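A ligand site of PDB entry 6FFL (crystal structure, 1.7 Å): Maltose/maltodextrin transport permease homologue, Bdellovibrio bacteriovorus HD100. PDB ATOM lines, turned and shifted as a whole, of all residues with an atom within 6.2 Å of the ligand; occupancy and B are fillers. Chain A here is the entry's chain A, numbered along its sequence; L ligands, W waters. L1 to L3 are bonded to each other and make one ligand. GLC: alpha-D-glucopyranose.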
ATOM      1  N   GLN A  10      11.534  14.701  -1.560  1.00  0.00           N
ATOM      2  CA  GLN A  10      12.248  15.977  -1.522  1.00  0.00           C
ATOM      3  C   GLN A  10      13.693  15.826  -2.023  1.00  0.00           C
ATOM      4  O   GLN A  10      14.610  16.505  -1.541  1.00  0.00           O
ATOM      5  CB  GLN A  10      12.197  16.597  -0.116  1.00  0.00           C
ATOM      6  CG  GLN A  10      12.449  15.653   1.072  1.00  0.00           C
ATOM      7  CD  GLN A  10      13.891  15.166   1.104  1.00  0.00           C
ATOM      8  OE1 GLN A  10      14.229  14.145   0.494  1.00  0.00           O
ATOM      9  NE2 GLN A  10      14.760  15.916   1.796  1.00  0.00           N
ATOM     10  N   MET A  11      13.896  14.968  -3.021  1.00  0.00           N
ATOM     11  CA  MET A  11      15.237  14.665  -3.514  1.00  0.00           C
ATOM     12  C   MET A  11      15.790  15.763  -4.422  1.00  0.00           C
ATOM     13  O   MET A  11      15.152  16.140  -5.412  1.00  0.00           O
ATOM     14  CB  MET A  11      15.249  13.345  -4.297  1.00  0.00           C
ATOM     15  CG  MET A  11      14.956  12.132  -3.452  1.00  0.00           C
ATOM     16  SD  MET A  11      15.285  10.630  -4.409  1.00  0.00           S
ATOM     17  CE  MET A  11      14.508   9.408  -3.347  1.00  0.00           C
ATOM     18  N   ILE A  12      17.019  16.196  -4.113  1.00  0.00           N
ATOM     19  CA  ILE A  12      17.752  17.146  -4.926  1.00  0.00           C
ATOM     20  C   ILE A  12      18.019  16.565  -6.329  1.00  0.00           C
ATOM     21  O   ILE A  12      17.980  15.356  -6.553  1.00  0.00           O
ATOM     22  CB  ILE A  12      19.067  17.476  -4.204  1.00  0.00           C
ATOM     23  CG1 ILE A  12      19.719  18.746  -4.739  1.00  0.00           C
ATOM     24  CG2 ILE A  12      20.040  16.290  -4.290  1.00  0.00           C
ATOM     25  CD1 ILE A  12      21.043  19.042  -4.040  1.00  0.00           C
ATOM     26  N   HIS A  15      20.021  13.353  -6.956  1.00  0.00           N
ATOM     27  CA  HIS A  15      19.389  12.168  -6.379  1.00  0.00           C
ATOM     28  C   HIS A  15      18.104  11.816  -7.121  1.00  0.00           C
ATOM     29  O   HIS A  15      17.805  10.633  -7.335  1.00  0.00           O
ATOM     30  CB  HIS A  15      19.073  12.385  -4.892  1.00  0.00           C
ATOM     31  CG  HIS A  15      20.288  12.408  -4.014  1.00  0.00           C
ATOM     32  ND1 HIS A  15      20.314  11.855  -2.757  1.00  0.00           N
ATOM     33  CD2 HIS A  15      21.521  12.942  -4.220  1.00  0.00           C
ATOM     34  CE1 HIS A  15      21.506  12.032  -2.222  1.00  0.00           C
ATOM     35  NE2 HIS A  15      22.258  12.694  -3.082  1.00  0.00           N
ATOM     36  N   TYR A  39       8.334  16.013  -6.897  1.00  0.00           N
ATOM     37  CA  TYR A  39       9.291  16.669  -6.008  1.00  0.00           C
ATOM     38  C   TYR A  39       8.604  17.813  -5.255  1.00  0.00           C
ATOM     39  O   TYR A  39       7.949  18.658  -5.865  1.00  0.00           O
ATOM     40  CB  TYR A  39      10.466  17.243  -6.802  1.00  0.00           C
ATOM     41  CG  TYR A  39      11.337  18.145  -5.943  1.00  0.00           C
ATOM     42  CD1 TYR A  39      12.297  17.611  -5.101  1.00  0.00           C
ATOM     43  CD2 TYR A  39      11.177  19.540  -5.957  1.00  0.00           C
ATOM     44  CE1 TYR A  39      13.082  18.411  -4.290  1.00  0.00           C
ATOM     45  CE2 TYR A  39      11.961  20.350  -5.142  1.00  0.00           C
ATOM     46  CZ  TYR A  39      12.908  19.779  -4.325  1.00  0.00           C
ATOM     47  OH  TYR A  39      13.691  20.571  -3.525  1.00  0.00           O
ATOM     48  N   GLU A  41       9.975  20.565  -2.028  1.00  0.00           N
ATOM     49  CA  GLU A  41      11.012  20.922  -1.082  1.00  0.00           C
ATOM     50  C   GLU A  41      10.604  20.443   0.304  1.00  0.00           C
ATOM     51  O   GLU A  41       9.412  20.394   0.627  1.00  0.00           O
ATOM     52  CB  GLU A  41      11.253  22.430  -1.089  1.00  0.00           C
ATOM     53  CG  GLU A  41      12.570  22.832  -0.399  1.00  0.00           C
ATOM     54  CD  GLU A  41      12.457  22.963   1.117  1.00  0.00           C
ATOM     55  OE1 GLU A  41      13.514  22.830   1.802  1.00  0.00           O
ATOM     56  OE2 GLU A  41      11.338  23.208   1.624  1.00  0.00           O
ATOM     57  N   THR A  42      11.607  20.089   1.118  1.00  0.00           N
ATOM     58  CA  THR A  42      11.406  19.423   2.408  1.00  0.00           C
ATOM     59  C   THR A  42      10.254  19.980   3.246  1.00  0.00           C
ATOM     60  O   THR A  42       9.395  19.216   3.707  1.00  0.00           O
ATOM     61  CB  THR A  42      12.717  19.503   3.204  1.00  0.00           C
ATOM     62  OG1 THR A  42      13.684  18.650   2.589  1.00  0.00           O
ATOM     63  CG2 THR A  42      12.509  19.063   4.659  1.00  0.00           C
ATOM     64  N   GLU A  43      10.216  21.296   3.462  1.00  0.00           N
ATOM     65  CA  GLU A  43       9.143  21.883   4.268  1.00  0.00           C
ATOM     66  C   GLU A  43       7.787  21.688   3.606  1.00  0.00           C
ATOM     67  O   GLU A  43       6.821  21.294   4.266  1.00  0.00           O
ATOM     68  CB  GLU A  43       9.426  23.374   4.497  1.00  0.00           C
ATOM     69  CG  GLU A  43      10.824  23.645   5.018  1.00  0.00           C
ATOM     70  CD  GLU A  43      11.083  22.940   6.332  1.00  0.00           C
ATOM     71  OE1 GLU A  43      12.139  22.290   6.465  1.00  0.00           O
ATOM     72  OE2 GLU A  43      10.234  23.056   7.245  1.00  0.00           O
ATOM     73  N   ARG A  46       6.467  18.054   3.783  1.00  0.00           N
ATOM     74  CA  ARG A  46       5.824  17.731   5.059  1.00  0.00           C
ATOM     75  C   ARG A  46       4.413  18.302   5.119  1.00  0.00           C
ATOM     76  O   ARG A  46       3.457  17.582   5.410  1.00  0.00           O
ATOM     77  CB  ARG A  46       6.664  18.265   6.219  1.00  0.00           C
ATOM     78  CG  ARG A  46       6.012  18.018   7.594  1.00  0.00           C
ATOM     79  CD  ARG A  46       6.755  18.743   8.696  1.00  0.00           C
ATOM     80  NE  ARG A  46       6.633  20.193   8.573  1.00  0.00           N
ATOM     81  CZ  ARG A  46       7.593  21.005   8.140  1.00  0.00           C
ATOM     82  NH1 ARG A  46       8.773  20.508   7.778  1.00  0.00           N
ATOM     83  NH2 ARG A  46       7.379  22.311   8.079  1.00  0.00           N
ATOM     84  N   PRO A  65      13.140  13.403   5.381  1.00  0.00           N
ATOM     85  CA  PRO A  65      14.021  13.227   6.554  1.00  0.00           C
ATOM     86  C   PRO A  65      13.318  12.514   7.698  1.00  0.00           C
ATOM     87  O   PRO A  65      12.098  12.592   7.855  1.00  0.00           O
ATOM     88  CB  PRO A  65      14.380  14.671   6.952  1.00  0.00           C
ATOM     89  CG  PRO A  65      13.960  15.541   5.798  1.00  0.00           C
ATOM     90  CD  PRO A  65      12.873  14.816   5.061  1.00  0.00           C
ATOM     91  N   SER A  66      14.114  11.847   8.525  1.00  0.00           N
ATOM     92  CA  SER A  66      13.535  10.971   9.527  1.00  0.00           C
ATOM     93  C   SER A  66      12.719  11.699  10.587  1.00  0.00           C
ATOM     94  O   SER A  66      11.861  11.061  11.198  1.00  0.00           O
ATOM     95  CB  SER A  66      14.617  10.127  10.186  1.00  0.00           C
ATOM     96  OG  SER A  66      15.658  10.943  10.647  1.00  0.00           O
ATOM     97  N   ASP A  67      12.953  13.003  10.825  1.00  0.00           N
ATOM     98  CA  ASP A  67      12.118  13.637  11.840  1.00  0.00           C
ATOM     99  C   ASP A  67      10.681  13.812  11.387  1.00  0.00           C
ATOM    100  O   ASP A  67       9.826  14.160  12.216  1.00  0.00           O
ATOM    101  CB  ASP A  67      12.721  14.969  12.343  1.00  0.00           C
ATOM    102  CG  ASP A  67      12.920  15.993  11.231  1.00  0.00           C
ATOM    103  OD1 ASP A  67      12.709  17.199  11.499  1.00  0.00           O
ATOM    104  OD2 ASP A  67      13.359  15.604  10.124  1.00  0.00           O
ATOM    105  N   GLN A  68      10.351  13.531  10.128  1.00  0.00           N
ATOM    106  CA  GLN A  68       8.921  13.634   9.827  1.00  0.00           C
ATOM    107  C   GLN A  68       8.133  12.446  10.379  1.00  0.00           C
ATOM    108  O   GLN A  68       6.896  12.491  10.379  1.00  0.00           O
ATOM    109  CB  GLN A  68       8.704  13.844   8.320  1.00  0.00           C
ATOM    110  CG  GLN A  68       9.053  12.716   7.420  1.00  0.00           C
ATOM    111  CD  GLN A  68       9.106  13.128   5.957  1.00  0.00           C
ATOM    112  OE1 GLN A  68       9.275  14.300   5.619  1.00  0.00           O
ATOM    113  NE2 GLN A  68       8.952  12.167   5.082  1.00  0.00           N
ATOM    114  N   ASN A 114      22.756  12.458   5.919  1.00  0.00           N
ATOM    115  CA  ASN A 114      21.958  13.667   6.082  1.00  0.00           C
ATOM    116  C   ASN A 114      22.664  14.693   6.947  1.00  0.00           C
ATOM    117  O   ASN A 114      22.026  15.545   7.569  1.00  0.00           O
ATOM    118  CB  ASN A 114      20.573  13.338   6.646  1.00  0.00           C
ATOM    119  CG  ASN A 114      19.559  14.403   6.317  1.00  0.00           C
ATOM    120  OD1 ASN A 114      19.436  14.802   5.155  1.00  0.00           O
ATOM    121  ND2 ASN A 114      18.829  14.885   7.328  1.00  0.00           N
ATOM    122  N   ASN A 160      23.419  28.227   4.132  1.00  0.00           N
ATOM    123  CA  ASN A 160      22.030  28.604   4.335  1.00  0.00           C
ATOM    124  C   ASN A 160      21.808  28.862   5.829  1.00  0.00           C
ATOM    125  O   ASN A 160      21.069  28.156   6.515  1.00  0.00           O
ATOM    126  CB  ASN A 160      21.106  27.519   3.805  1.00  0.00           C
ATOM    127  CG  ASN A 160      19.655  27.923   3.806  1.00  0.00           C
ATOM    128  OD1 ASN A 160      19.331  29.118   3.866  1.00  0.00           O
ATOM    129  ND2 ASN A 160      18.757  26.940   3.750  1.00  0.00           N
ATOM    130  N   GLU A 163      18.472  28.951   8.032  1.00  0.00           N
ATOM    131  CA  GLU A 163      17.709  27.713   8.209  1.00  0.00           C
ATOM    132  C   GLU A 163      18.192  27.001   9.467  1.00  0.00           C
ATOM    133  O   GLU A 163      19.384  26.754   9.606  1.00  0.00           O
ATOM    134  CB  GLU A 163      17.898  26.822   6.984  1.00  0.00           C
ATOM    135  CG  GLU A 163      17.051  25.566   6.959  1.00  0.00           C
ATOM    136  CD  GLU A 163      15.574  25.833   6.875  1.00  0.00           C
ATOM    137  OE1 GLU A 163      15.183  26.853   6.251  1.00  0.00           O
ATOM    138  OE2 GLU A 163      14.768  25.046   7.441  1.00  0.00           O
ATOM    139  N   PRO A 164      17.296  26.643  10.406  1.00  0.00           N
ATOM    140  CA  PRO A 164      17.767  26.119  11.698  1.00  0.00           C
ATOM    141  C   PRO A 164      18.652  24.885  11.589  1.00  0.00           C
ATOM    142  O   PRO A 164      19.576  24.733  12.393  1.00  0.00           O
ATOM    143  CB  PRO A 164      16.467  25.814  12.441  1.00  0.00           C
ATOM    144  CG  PRO A 164      15.474  26.726  11.842  1.00  0.00           C
ATOM    145  CD  PRO A 164      15.844  26.902  10.399  1.00  0.00           C
ATOM    146  N   PHE A 165      18.388  23.995  10.635  1.00  0.00           N
ATOM    147  CA  PHE A 165      19.249  22.823  10.483  1.00  0.00           C
ATOM    148  C   PHE A 165      20.715  23.231  10.350  1.00  0.00           C
ATOM    149  O   PHE A 165      21.605  22.534  10.840  1.00  0.00           O
ATOM    150  CB  PHE A 165      18.809  22.025   9.261  1.00  0.00           C
ATOM    151  CG  PHE A 165      19.347  20.615   9.208  1.00  0.00           C
ATOM    152  CD1 PHE A 165      18.947  19.667  10.139  1.00  0.00           C
ATOM    153  CD2 PHE A 165      20.236  20.235   8.208  1.00  0.00           C
ATOM    154  CE1 PHE A 165      19.412  18.345  10.073  1.00  0.00           C
ATOM    155  CE2 PHE A 165      20.716  18.937   8.139  1.00  0.00           C
ATOM    156  CZ  PHE A 165      20.303  17.982   9.087  1.00  0.00           C
ATOM    157  N   PHE A 166      20.963  24.370   9.716  1.00  0.00           N
ATOM    158  CA  PHE A 166      22.328  24.773   9.405  1.00  0.00           C
ATOM    159  C   PHE A 166      23.026  25.475  10.569  1.00  0.00           C
ATOM    160  O   PHE A 166      24.260  25.518  10.589  1.00  0.00           O
ATOM    161  CB  PHE A 166      22.336  25.644   8.152  1.00  0.00           C
ATOM    162  CG  PHE A 166      22.016  24.873   6.888  1.00  0.00           C
ATOM    163  CD1 PHE A 166      20.710  24.515   6.576  1.00  0.00           C
ATOM    164  CD2 PHE A 166      23.043  24.495   6.024  1.00  0.00           C
ATOM    165  CE1 PHE A 166      20.421  23.795   5.409  1.00  0.00           C
ATOM    166  CE2 PHE A 166      22.754  23.775   4.857  1.00  0.00           C
ATOM    167  CZ  PHE A 166      21.450  23.434   4.559  1.00  0.00           C
ATOM    168  N   TYR A 216      19.657  28.830   0.335  1.00  0.00           N
ATOM    169  CA  TYR A 216      20.306  27.581  -0.058  1.00  0.00           C
ATOM    170  C   TYR A 216      20.844  27.668  -1.478  1.00  0.00           C
ATOM    171  O   TYR A 216      22.006  27.321  -1.744  1.00  0.00           O
ATOM    172  CB  TYR A 216      19.365  26.386   0.069  1.00  0.00           C
ATOM    173  CG  TYR A 216      20.072  25.089  -0.273  1.00  0.00           C
ATOM    174  CD1 TYR A 216      20.713  24.345   0.718  1.00  0.00           C
ATOM    175  CD2 TYR A 216      20.119  24.619  -1.577  1.00  0.00           C
ATOM    176  CE1 TYR A 216      21.376  23.149   0.409  1.00  0.00           C
ATOM    177  CE2 TYR A 216      20.780  23.437  -1.905  1.00  0.00           C
ATOM    178  CZ  TYR A 216      21.409  22.720  -0.902  1.00  0.00           C
ATOM    179  OH  TYR A 216      22.056  21.548  -1.232  1.00  0.00           O
ATOM    180  N   ASN A 233      27.318  22.352   3.944  1.00  0.00           N
ATOM    181  CA  ASN A 233      26.213  21.690   3.275  1.00  0.00           C
ATOM    182  C   ASN A 233      26.266  20.208   3.630  1.00  0.00           C
ATOM    183  O   ASN A 233      27.202  19.744   4.283  1.00  0.00           O
ATOM    184  CB  ASN A 233      26.274  21.912   1.745  1.00  0.00           C
ATOM    185  CG  ASN A 233      24.900  21.862   1.078  1.00  0.00           C
ATOM    186  OD1 ASN A 233      23.902  21.485   1.700  1.00  0.00           O
ATOM    187  ND2 ASN A 233      24.843  22.266  -0.184  1.00  0.00           N
ATOM    188  N   TRP A 236      23.863  15.151   0.830  1.00  0.00           N
ATOM    189  CA  TRP A 236      22.996  15.141  -0.343  1.00  0.00           C
ATOM    190  C   TRP A 236      23.555  15.972  -1.492  1.00  0.00           C
ATOM    191  O   TRP A 236      23.102  15.808  -2.631  1.00  0.00           O
ATOM    192  CB  TRP A 236      21.595  15.686   0.003  1.00  0.00           C
ATOM    193  CG  TRP A 236      21.664  17.089   0.560  1.00  0.00           C
ATOM    194  CD1 TRP A 236      21.786  18.251  -0.143  1.00  0.00           C
ATOM    195  CD2 TRP A 236      21.679  17.470   1.951  1.00  0.00           C
ATOM    196  NE1 TRP A 236      21.855  19.332   0.709  1.00  0.00           N
ATOM    197  CE2 TRP A 236      21.786  18.870   2.010  1.00  0.00           C
ATOM    198  CE3 TRP A 236      21.588  16.750   3.152  1.00  0.00           C
ATOM    199  CZ2 TRP A 236      21.815  19.576   3.213  1.00  0.00           C
ATOM    200  CZ3 TRP A 236      21.622  17.445   4.361  1.00  0.00           C
ATOM    201  CH2 TRP A 236      21.735  18.845   4.384  1.00  0.00           C
ATOM    202  N   THR A 269      18.704   9.827   8.463  1.00  0.00           N
ATOM    203  CA  THR A 269      18.382   9.265   7.164  1.00  0.00           C
ATOM    204  C   THR A 269      17.302  10.099   6.502  1.00  0.00           C
ATOM    205  O   THR A 269      16.705  10.992   7.112  1.00  0.00           O
ATOM    206  CB  THR A 269      17.929   7.788   7.294  1.00  0.00           C
ATOM    207  OG1 THR A 269      17.953   7.165   6.003  1.00  0.00           O
ATOM    208  CG2 THR A 269      16.511   7.693   7.867  1.00  0.00           C
ATOM    209  N   LYS A 270      17.059   9.811   5.232  1.00  0.00           N
ATOM    210  CA  LYS A 270      15.816  10.167   4.562  1.00  0.00           C
ATOM    211  C   LYS A 270      15.238   8.867   4.031  1.00  0.00           C
ATOM    212  O   LYS A 270      15.973   8.036   3.489  1.00  0.00           O
ATOM    213  CB  LYS A 270      16.066  11.191   3.436  1.00  0.00           C
ATOM    214  CG  LYS A 270      16.677  12.525   3.936  1.00  0.00           C
ATOM    215  CD  LYS A 270      17.103  13.415   2.774  1.00  0.00           C
ATOM    216  CE  LYS A 270      18.399  12.905   2.135  1.00  0.00           C
ATOM    217  NZ  LYS A 270      19.565  12.901   3.088  1.00  0.00           N
ATOM    218  N   MET A 341      19.544  12.283  14.700  1.00  0.00           N
ATOM    219  CA  MET A 341      18.391  13.132  14.441  1.00  0.00           C
ATOM    220  C   MET A 341      17.236  12.728  15.352  1.00  0.00           C
ATOM    221  O   MET A 341      16.839  11.547  15.347  1.00  0.00           O
ATOM    222  CB  MET A 341      17.965  13.009  12.979  1.00  0.00           C
ATOM    223  CG  MET A 341      16.715  13.801  12.620  1.00  0.00           C
ATOM    224  SD  MET A 341      17.100  15.577  12.586  1.00  0.00           S
ATOM    225  CE  MET A 341      16.565  16.035  10.936  1.00  0.00           C
ATOM    226  N   ARG A 348       9.441  19.189  15.784  1.00  0.00           N
ATOM    227  CA  ARG A 348       8.824  20.070  14.799  1.00  0.00           C
ATOM    228  C   ARG A 348       8.587  21.455  15.391  1.00  0.00           C
ATOM    229  O   ARG A 348       8.854  22.477  14.734  1.00  0.00           O
ATOM    230  CB  ARG A 348       7.504  19.441  14.324  1.00  0.00           C
ATOM    231  CG  ARG A 348       6.671  20.319  13.434  1.00  0.00           C
ATOM    232  CD  ARG A 348       7.189  20.267  12.017  1.00  0.00           C
ATOM    233  NE  ARG A 348       8.042  21.413  11.686  1.00  0.00           N
ATOM    234  CZ  ARG A 348       9.250  21.298  11.128  1.00  0.00           C
ATOM    235  NH1 ARG A 348       9.748  20.111  10.858  1.00  0.00           N
ATOM    236  NH2 ARG A 348       9.923  22.393  10.819  1.00  0.00           N
ATOM    237  N   TRP A 351      12.000  23.240  15.601  1.00  0.00           N
ATOM    238  CA  TRP A 351      12.444  23.800  14.316  1.00  0.00           C
ATOM    239  C   TRP A 351      11.661  25.051  13.957  1.00  0.00           C
ATOM    240  O   TRP A 351      12.226  26.047  13.499  1.00  0.00           O
ATOM    241  CB  TRP A 351      12.289  22.771  13.199  1.00  0.00           C
ATOM    242  CG  TRP A 351      13.176  21.584  13.224  1.00  0.00           C
ATOM    243  CD1 TRP A 351      12.800  20.292  13.026  1.00  0.00           C
ATOM    244  CD2 TRP A 351      14.615  21.562  13.389  1.00  0.00           C
ATOM    245  NE1 TRP A 351      13.899  19.462  13.076  1.00  0.00           N
ATOM    246  CE2 TRP A 351      15.020  20.217  13.302  1.00  0.00           C
ATOM    247  CE3 TRP A 351      15.586  22.549  13.613  1.00  0.00           C
ATOM    248  CZ2 TRP A 351      16.348  19.824  13.434  1.00  0.00           C
ATOM    249  CZ3 TRP A 351      16.913  22.155  13.745  1.00  0.00           C
ATOM    250  CH2 TRP A 351      17.284  20.808  13.652  1.00  0.00           C
ATOM    251  N   ASP A 352      10.330  24.986  14.084  1.00  0.00           N
ATOM    252  CA  ASP A 352       9.511  26.117  13.649  1.00  0.00           C
ATOM    253  C   ASP A 352       9.754  27.356  14.505  1.00  0.00           C
ATOM    254  O   ASP A 352       9.811  28.470  13.983  1.00  0.00           O
ATOM    255  CB  ASP A 352       8.029  25.724  13.679  1.00  0.00           C
ATOM    256  CG  ASP A 352       7.677  24.714  12.585  1.00  0.00           C
ATOM    257  OD1 ASP A 352       8.412  24.637  11.589  1.00  0.00           O
ATOM    258  OD2 ASP A 352       6.667  23.996  12.732  1.00  0.00           O
ATOM    259  N   ARG A 355      13.205  28.888  13.643  1.00  0.00           N
ATOM    260  CA  ARG A 355      13.244  29.619  12.379  1.00  0.00           C
ATOM    261  C   ARG A 355      12.619  31.002  12.527  1.00  0.00           C
ATOM    262  O   ARG A 355      13.160  31.984  12.032  1.00  0.00           O
ATOM    263  CB  ARG A 355      12.540  28.836  11.281  1.00  0.00           C
ATOM    264  CG  ARG A 355      12.774  29.409   9.886  1.00  0.00           C
ATOM    265  CD  ARG A 355      11.908  28.718   8.831  1.00  0.00           C
ATOM    266  NE  ARG A 355      12.266  27.313   8.675  1.00  0.00           N
ATOM    267  CZ  ARG A 355      11.537  26.295   9.131  1.00  0.00           C
ATOM    268  NH1 ARG A 355      10.388  26.523   9.762  1.00  0.00           N
ATOM    269  NH2 ARG A 355      11.948  25.054   8.938  1.00  0.00           N
HETATM  270  C1  GLC L   1      17.730  18.985  -1.186  1.00  0.00           C
HETATM  271  C2  GLC L   1      17.950  17.646  -0.475  1.00  0.00           C
HETATM  272  C3  GLC L   1      17.415  17.684   0.948  1.00  0.00           C
HETATM  273  C4  GLC L   1      17.944  18.906   1.703  1.00  0.00           C
HETATM  274  C5  GLC L   1      17.686  20.182   0.895  1.00  0.00           C
HETATM  275  C6  GLC L   1      18.327  21.399   1.571  1.00  0.00           C
HETATM  276  O1  GLC L   1      16.334  19.195  -1.402  1.00  0.00           O
HETATM  277  O2  GLC L   1      17.248  16.603  -1.163  1.00  0.00           O
HETATM  278  O3  GLC L   1      17.777  16.451   1.611  1.00  0.00           O
HETATM  279  O4  GLC L   1      17.279  18.944   2.986  1.00  0.00           O
HETATM  280  O5  GLC L   1      18.255  20.085  -0.409  1.00  0.00           O
HETATM  281  O6  GLC L   1      17.943  22.602   0.890  1.00  0.00           O
HETATM  282  C1  GLC L   2      18.240  18.972   4.025  1.00  0.00           C
HETATM  283  C2  GLC L   2      18.013  17.842   5.015  1.00  0.00           C
HETATM  284  C3  GLC L   2      16.763  18.049   5.862  1.00  0.00           C
HETATM  285  C4  GLC L   2      16.832  19.434   6.483  1.00  0.00           C
HETATM  286  C5  GLC L   2      16.974  20.480   5.382  1.00  0.00           C
HETATM  287  C6  GLC L   2      17.036  21.898   5.956  1.00  0.00           C
HETATM  288  O2  GLC L   2      17.930  16.614   4.274  1.00  0.00           O
HETATM  289  O3  GLC L   2      16.736  17.040   6.891  1.00  0.00           O
HETATM  290  O4  GLC L   2      15.631  19.696   7.193  1.00  0.00           O
HETATM  291  O5  GLC L   2      18.192  20.226   4.688  1.00  0.00           O
HETATM  292  O6  GLC L   2      16.807  22.868   4.910  1.00  0.00           O
HETATM  293  C1  GLC L   3      15.750  19.513   8.596  1.00  0.00           C
HETATM  294  C2  GLC L   3      14.550  18.721   9.106  1.00  0.00           C
HETATM  295  C3  GLC L   3      13.271  19.527   8.867  1.00  0.00           C
HETATM  296  C4  GLC L   3      13.377  20.885   9.532  1.00  0.00           C
HETATM  297  C5  GLC L   3      14.625  21.621   9.020  1.00  0.00           C
HETATM  298  C6  GLC L   3      14.853  22.890   9.833  1.00  0.00           C
HETATM  299  O2  GLC L   3      14.475  17.432   8.475  1.00  0.00           O
HETATM  300  O3  GLC L   3      12.135  18.826   9.422  1.00  0.00           O
HETATM  301  O4  GLC L   3      12.205  21.656   9.209  1.00  0.00           O
HETATM  302  O5  GLC L   3      15.776  20.792   9.238  1.00  0.00           O
HETATM  303  O6  GLC L   3      15.851  23.743   9.231  1.00  0.00           O
HETATM  304  O   HOH W   1       9.946  17.925   7.923  1.00  0.00           O
HETATM  305  O   HOH W   2      15.550  22.647   0.488  1.00  0.00           O
HETATM  306  O   HOH W   3      17.951  24.304   2.949  1.00  0.00           O
HETATM  307  O   HOH W   4      16.334  20.327  -3.835  1.00  0.00           O
HETATM  308  O   HOH W   5      14.320  19.922  -0.155  1.00  0.00           O
HETATM  309  O   HOH W   6      14.061  22.941   4.690  1.00  0.00           O
HETATM  310  O   HOH W   7      16.699  13.734  -0.505  1.00  0.00           O
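The backbone nitrogen of Pro 164 lies close to an oxygen (O6) of GLC L3 (3.4 Å).
Merely in contact with the ligand: Met 11, Tyr 39, Thr 42, Arg 46, Pro 65, Phe 166, Tyr 216, Trp 236, Lys 270, Met 341 and Trp 351.
Hydrophobic or aromatic side chains that line the ligand: Ile 12, Pro 65, Pro 164, Phe 165, Phe 166, Tyr 216, Trp 236, Met 341 and Trp 351.
The side-chain carboxylate (OE2) of Glu 163 sits at hydrogen-bond distance from an oxygen (O6) of GLC L3, at 2.5 Å.
OD1 of Asn 114 lies within hydrogen-bond range of O2 of GLC L2, at 2.5 Å.
The backbone carbonyl oxygen of Gln 10 is in hydrogen-bond range of an oxygen (O2) of GLC L1, 2.7 Å away.
The side-chain amide nitrogen (NE2) of Gln 10 sits at hydrogen-bond distance from an oxygen (O3) of GLC L1, 3.1 Å away.
OD1 of Asp 67 is in hydrogen-bond range of O3 of GLC L3 (2.7 Å).
The side-chain carboxylate (OE1) of Glu 43 lies within hydrogen-bond range of an oxygen (O4) of GLC L3, at 2.8 Å.
The guanidinium group of Arg 348 is in hydrogen-bond range of an oxygen (O4) of GLC L3 (2.9 Å).
N of Phe 165 lies within hydrogen-bond range of O6 of GLC L3 (2.9 Å).
An oxygen (O2) of GLC L1 lies within hydrogen-bond range of the backbone NH of Ile 12, 3.0 Å away.
The guanidinium group of Arg 355 is in hydrogen-bond range of an oxygen (O4) of GLC L3, 3.4 Å away.
Water W2 lies within hydrogen-bond range of an oxygen (O6) of GLC L1 (2.4 Å) and the side-chain carboxylate (OE1) of Glu 41 (2.4 Å).
Water W5 lies within hydrogen-bond range of an oxygen (O1) of GLC L1 (2.5 Å), the backbone NH (N) of Thr 42 (3.0 Å) and the side-chain hydroxyl (OH) of Tyr 39 (3.5 Å).
Water W4 lies within hydrogen-bond range of the side-chain hydroxyl (OH) of Tyr 39 and an oxygen (O1) of GLC L1.
Water W6 lies within hydrogen-bond range of the side-chain carboxylate (OE1) of Glu 43 (2.7 Å), an oxygen (O6) of GLC L2 (2.8 Å) and the side-chain carboxylate (OE1) of Glu 41 (2.9 Å).
Water W1 lies within hydrogen-bond range of an oxygen (O3) of GLC L3 (2.8 Å) and the guanidinium group of Arg 46 (2.8 Å).
Water W7 lies within hydrogen-bond range of OE1 of Gln 10 (2.7 Å) and O2 of GLC L1 (3.0 Å).
The guanidinium group (NH2) of Arg 355 is in salt-bridge range of the side-chain carboxylate (OE2) of Glu 163.
The guanidinium group (NH2) of Arg 348 is in salt-bridge range of the side-chain carboxylate (OE2) of Glu 43 (3.6 Å).
The side-chain carboxylate (OE2) of Glu 43 is in salt-bridge range of the guanidinium group (NH2) of Arg 355 (3.1 Å).
N of Glu 43 sits at hydrogen-bond distance from OE2 of Glu 41, 2.9 Å away.
The side-chain amide nitrogen of Asn 233 is in hydrogen-bond range of the side-chain hydroxyl of Tyr 216 (3.1 Å).
OD1 of Asp 352 is in salt-bridge range of NH1 of Arg 355, at 3.3 Å.
OD1 of Asn 233 sits at hydrogen-bond distance from NE1 of Trp 236, at 3.1 Å.
A ring nitrogen (NE2) of His 15 sits at hydrogen-bond distance from the backbone carbonyl oxygen (O) of Trp 236 (3.3 Å).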
